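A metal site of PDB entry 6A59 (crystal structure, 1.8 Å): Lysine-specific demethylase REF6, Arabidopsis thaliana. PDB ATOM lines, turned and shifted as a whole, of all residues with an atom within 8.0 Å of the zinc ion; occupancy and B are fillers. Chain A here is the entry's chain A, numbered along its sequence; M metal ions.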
ATOM      1  N   LYS A  77      32.398  23.907  -8.999  1.00  0.00           N
ATOM      2  CA  LYS A  77      31.825  24.264  -7.701  1.00  0.00           C
ATOM      3  C   LYS A  77      31.560  25.759  -7.605  1.00  0.00           C
ATOM      4  O   LYS A  77      32.315  26.556  -8.174  1.00  0.00           O
ATOM      5  CB  LYS A  77      32.774  23.854  -6.557  1.00  0.00           C
ATOM      6  CG  LYS A  77      33.131  22.382  -6.522  1.00  0.00           C
ATOM      7  CD  LYS A  77      33.753  22.008  -5.184  1.00  0.00           C
ATOM      8  CE  LYS A  77      34.174  20.546  -5.121  1.00  0.00           C
ATOM      9  NZ  LYS A  77      35.471  20.290  -5.819  1.00  0.00           N
ATOM     10  N   CYS A  78      30.511  26.139  -6.884  1.00  0.00           N
ATOM     11  CA  CYS A  78      30.238  27.543  -6.605  1.00  0.00           C
ATOM     12  C   CYS A  78      31.349  28.122  -5.718  1.00  0.00           C
ATOM     13  O   CYS A  78      31.723  27.488  -4.721  1.00  0.00           O
ATOM     14  CB  CYS A  78      28.889  27.705  -5.902  1.00  0.00           C
ATOM     15  SG  CYS A  78      28.461  29.436  -5.530  1.00  0.00           S
ATOM     16  N   PRO A  79      31.882  29.310  -6.061  1.00  0.00           N
ATOM     17  CA  PRO A  79      32.941  29.924  -5.259  1.00  0.00           C
ATOM     18  C   PRO A  79      32.482  30.656  -3.989  1.00  0.00           C
ATOM     19  O   PRO A  79      33.330  31.150  -3.244  1.00  0.00           O
ATOM     20  CB  PRO A  79      33.574  30.908  -6.239  1.00  0.00           C
ATOM     21  CG  PRO A  79      32.426  31.358  -7.062  1.00  0.00           C
ATOM     22  CD  PRO A  79      31.565  30.141  -7.242  1.00  0.00           C
ATOM     23  N   TRP A  80      31.173  30.733  -3.741  1.00  0.00           N
ATOM     24  CA  TRP A  80      30.627  31.467  -2.599  1.00  0.00           C
ATOM     25  C   TRP A  80      30.734  30.601  -1.339  1.00  0.00           C
ATOM     26  O   TRP A  80      30.186  29.505  -1.309  1.00  0.00           O
ATOM     27  CB  TRP A  80      29.156  31.822  -2.872  1.00  0.00           C
ATOM     28  CG  TRP A  80      28.656  33.038  -2.179  1.00  0.00           C
ATOM     29  CD1 TRP A  80      27.810  33.080  -1.101  1.00  0.00           C
ATOM     30  CD2 TRP A  80      28.937  34.391  -2.525  1.00  0.00           C
ATOM     31  NE1 TRP A  80      27.558  34.382  -0.758  1.00  0.00           N
ATOM     32  CE2 TRP A  80      28.241  35.210  -1.603  1.00  0.00           C
ATOM     33  CE3 TRP A  80      29.718  35.002  -3.519  1.00  0.00           C
ATOM     34  CZ2 TRP A  80      28.298  36.609  -1.660  1.00  0.00           C
ATOM     35  CZ3 TRP A  80      29.777  36.392  -3.572  1.00  0.00           C
ATOM     36  CH2 TRP A  80      29.066  37.179  -2.643  1.00  0.00           C
ATOM     37  N   LYS A  81      31.448  31.091  -0.326  1.00  0.00           N
ATOM     38  CA  LYS A  81      31.628  30.329   0.920  1.00  0.00           C
ATOM     39  C   LYS A  81      30.287  29.966   1.553  1.00  0.00           C
ATOM     40  O   LYS A  81      29.372  30.788   1.579  1.00  0.00           O
ATOM     41  CB  LYS A  81      32.486  31.100   1.925  1.00  0.00           C
ATOM     42  CG  LYS A  81      33.957  31.223   1.537  1.00  0.00           C
ATOM     43  CD  LYS A  81      34.848  31.518   2.728  1.00  0.00           C
ATOM     44  CE  LYS A  81      34.506  32.823   3.418  1.00  0.00           C
ATOM     45  NZ  LYS A  81      35.496  33.179   4.475  1.00  0.00           N
ATOM     46  N   GLY A  82      30.175  28.718   2.015  1.00  0.00           N
ATOM     47  CA  GLY A  82      28.920  28.186   2.546  1.00  0.00           C
ATOM     48  C   GLY A  82      28.055  27.446   1.539  1.00  0.00           C
ATOM     49  O   GLY A  82      27.289  26.564   1.924  1.00  0.00           O
ATOM     50  N   CYS A  83      28.165  27.801   0.248  1.00  0.00           N
ATOM     51  CA  CYS A  83      27.354  27.191  -0.809  1.00  0.00           C
ATOM     52  C   CYS A  83      27.998  25.900  -1.310  1.00  0.00           C
ATOM     53  O   CYS A  83      29.193  25.877  -1.624  1.00  0.00           O
ATOM     54  CB  CYS A  83      27.156  28.159  -1.967  1.00  0.00           C
ATOM     55  SG  CYS A  83      26.040  27.532  -3.246  1.00  0.00           S
ATOM     56  N   LYS A  84      27.193  24.838  -1.393  1.00  0.00           N
ATOM     57  CA  LYS A  84      27.662  23.510  -1.781  1.00  0.00           C
ATOM     58  C   LYS A  84      27.215  23.119  -3.197  1.00  0.00           C
ATOM     59  O   LYS A  84      27.420  21.988  -3.614  1.00  0.00           O
ATOM     60  CB  LYS A  84      27.163  22.470  -0.772  1.00  0.00           C
ATOM     61  CG  LYS A  84      27.581  22.745   0.664  1.00  0.00           C
ATOM     62  CD  LYS A  84      27.021  21.698   1.623  1.00  0.00           C
ATOM     63  CE  LYS A  84      27.350  22.027   3.068  1.00  0.00           C
ATOM     64  NZ  LYS A  84      26.905  20.967   4.001  1.00  0.00           N
ATOM     65  N   MET A  85      26.631  24.071  -3.940  1.00  0.00           N
ATOM     66  CA  MET A  85      26.101  23.767  -5.269  1.00  0.00           C
ATOM     67  C   MET A  85      27.212  23.582  -6.292  1.00  0.00           C
ATOM     68  O   MET A  85      28.261  24.222  -6.219  1.00  0.00           O
ATOM     69  CB  MET A  85      25.127  24.851  -5.738  1.00  0.00           C
ATOM     70  CG  MET A  85      23.822  24.873  -4.940  1.00  0.00           C
ATOM     71  SD  MET A  85      22.433  25.511  -5.881  1.00  0.00           S
ATOM     72  CE  MET A  85      22.141  24.164  -7.029  1.00  0.00           C
ATOM     73  N   THR A  86      26.953  22.687  -7.244  1.00  0.00           N
ATOM     74  CA  THR A  86      27.905  22.323  -8.299  1.00  0.00           C
ATOM     75  C   THR A  86      27.199  22.364  -9.648  1.00  0.00           C
ATOM     76  O   THR A  86      25.976  22.253  -9.716  1.00  0.00           O
ATOM     77  CB  THR A  86      28.482  20.930  -8.068  1.00  0.00           C
ATOM     78  OG1 THR A  86      27.408  19.993  -7.893  1.00  0.00           O
ATOM     79  CG2 THR A  86      29.364  20.917  -6.829  1.00  0.00           C
ATOM     80  N   PHE A  87      27.981  22.532 -10.719  1.00  0.00           N
ATOM     81  CA  PHE A  87      27.437  22.764 -12.062  1.00  0.00           C
ATOM     82  C   PHE A  87      28.202  22.032 -13.147  1.00  0.00           C
ATOM     83  O   PHE A  87      29.396  21.758 -12.999  1.00  0.00           O
ATOM     84  CB  PHE A  87      27.427  24.267 -12.352  1.00  0.00           C
ATOM     85  CG  PHE A  87      26.647  25.042 -11.341  1.00  0.00           C
ATOM     86  CD1 PHE A  87      25.279  25.180 -11.463  1.00  0.00           C
ATOM     87  CD2 PHE A  87      27.274  25.565 -10.212  1.00  0.00           C
ATOM     88  CE1 PHE A  87      24.545  25.866 -10.506  1.00  0.00           C
ATOM     89  CE2 PHE A  87      26.550  26.244  -9.249  1.00  0.00           C
ATOM     90  CZ  PHE A  87      25.185  26.394  -9.396  1.00  0.00           C
ATOM     91  N   ARG A  93      26.928  28.146 -13.638  1.00  0.00           N
ATOM     92  CA  ARG A  93      27.592  28.611 -12.422  1.00  0.00           C
ATOM     93  C   ARG A  93      27.584  30.143 -12.336  1.00  0.00           C
ATOM     94  O   ARG A  93      27.253  30.697 -11.296  1.00  0.00           O
ATOM     95  CB  ARG A  93      29.036  28.096 -12.322  1.00  0.00           C
ATOM     96  CG  ARG A  93      29.782  28.616 -11.111  1.00  0.00           C
ATOM     97  CD  ARG A  93      31.059  27.851 -10.834  1.00  0.00           C
ATOM     98  NE  ARG A  93      32.068  28.054 -11.879  1.00  0.00           N
ATOM     99  CZ  ARG A  93      33.306  27.572 -11.834  1.00  0.00           C
ATOM    100  NH1 ARG A  93      33.731  26.828 -10.804  1.00  0.00           N
ATOM    101  NH2 ARG A  93      34.141  27.814 -12.848  1.00  0.00           N
ATOM    102  N   HIS A  96      24.196  31.349 -11.505  1.00  0.00           N
ATOM    103  CA  HIS A  96      23.910  31.044 -10.099  1.00  0.00           C
ATOM    104  C   HIS A  96      24.522  32.026  -9.122  1.00  0.00           C
ATOM    105  O   HIS A  96      23.876  32.403  -8.130  1.00  0.00           O
ATOM    106  CB  HIS A  96      24.378  29.651  -9.714  1.00  0.00           C
ATOM    107  CG  HIS A  96      24.143  29.324  -8.274  1.00  0.00           C
ATOM    108  ND1 HIS A  96      22.877  29.153  -7.761  1.00  0.00           N
ATOM    109  CD2 HIS A  96      24.997  29.176  -7.228  1.00  0.00           C
ATOM    110  CE1 HIS A  96      22.956  28.890  -6.476  1.00  0.00           C
ATOM    111  NE2 HIS A  96      24.226  28.892  -6.124  1.00  0.00           N
ATOM    112  N   ILE A  97      25.766  32.435  -9.382  1.00  0.00           N
ATOM    113  CA  ILE A  97      26.481  33.377  -8.491  1.00  0.00           C
ATOM    114  C   ILE A  97      25.713  34.704  -8.318  1.00  0.00           C
ATOM    115  O   ILE A  97      25.804  35.322  -7.256  1.00  0.00           O
ATOM    116  CB  ILE A  97      27.938  33.601  -8.974  1.00  0.00           C
ATOM    117  CG1 ILE A  97      28.756  32.310  -8.802  1.00  0.00           C
ATOM    118  CG2 ILE A  97      28.624  34.722  -8.198  1.00  0.00           C
ATOM    119  CD1 ILE A  97      29.958  32.214  -9.717  1.00  0.00           C
ATOM    120  N   ARG A  98      24.951  35.103  -9.344  1.00  0.00           N
ATOM    121  CA  ARG A  98      24.087  36.295  -9.254  1.00  0.00           C
ATOM    122  C   ARG A  98      23.054  36.232  -8.120  1.00  0.00           C
ATOM    123  O   ARG A  98      22.679  37.262  -7.590  1.00  0.00           O
ATOM    124  CB  ARG A  98      23.350  36.552 -10.565  1.00  0.00           C
ATOM    125  CG  ARG A  98      24.275  36.931 -11.709  1.00  0.00           C
ATOM    126  CD  ARG A  98      23.534  36.965 -13.033  1.00  0.00           C
ATOM    127  NE  ARG A  98      24.468  36.987 -14.150  1.00  0.00           N
ATOM    128  CZ  ARG A  98      24.160  36.710 -15.419  1.00  0.00           C
ATOM    129  NH1 ARG A  98      22.920  36.367 -15.765  1.00  0.00           N
ATOM    130  NH2 ARG A  98      25.109  36.753 -16.351  1.00  0.00           N
ATOM    131  N   VAL A  99      22.620  35.019  -7.771  1.00  0.00           N
ATOM    132  CA  VAL A  99      21.683  34.828  -6.641  1.00  0.00           C
ATOM    133  C   VAL A  99      22.345  35.314  -5.344  1.00  0.00           C
ATOM    134  O   VAL A  99      21.696  35.940  -4.517  1.00  0.00           O
ATOM    135  CB  VAL A  99      21.245  33.343  -6.485  1.00  0.00           C
ATOM    136  CG1 VAL A  99      20.340  33.158  -5.270  1.00  0.00           C
ATOM    137  CG2 VAL A  99      20.547  32.844  -7.745  1.00  0.00           C
ATOM    138  N   HIS A 100      23.630  35.012  -5.192  1.00  0.00           N
ATOM    139  CA  HIS A 100      24.412  35.439  -4.036  1.00  0.00           C
ATOM    140  C   HIS A 100      24.746  36.939  -4.031  1.00  0.00           C
ATOM    141  O   HIS A 100      24.658  37.576  -2.987  1.00  0.00           O
ATOM    142  CB  HIS A 100      25.699  34.617  -3.935  1.00  0.00           C
ATOM    143  CG  HIS A 100      25.472  33.182  -3.599  1.00  0.00           C
ATOM    144  ND1 HIS A 100      24.802  32.797  -2.461  1.00  0.00           N
ATOM    145  CD2 HIS A 100      25.798  32.032  -4.247  1.00  0.00           C
ATOM    146  CE1 HIS A 100      24.737  31.480  -2.413  1.00  0.00           C
ATOM    147  NE2 HIS A 100      25.333  30.990  -3.481  1.00  0.00           N
HETATM  148 ZN    ZN M   1      26.433  29.182  -4.730  1.00  0.00          ZN
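NE2 of His 96 lies close to SG of Cys 83 (3.7 Å).
O of Met 85 sits at hydrogen-bond distance from N of Cys 78 (3.0 Å).
N of Met 85 lies close to SG of Cys 83, 3.6 Å away.
The side-chain sulfur of Cys 78 sits close to the backbone NH of Trp 80.
The zinc ion is bound by SG of Cys 78, SG of Cys 83 and NE2 of His 100.
The zinc ion has three donor atoms within binding distance.
Slightly farther from the zinc ion lies NE2 of His 96 (2.6 Å).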
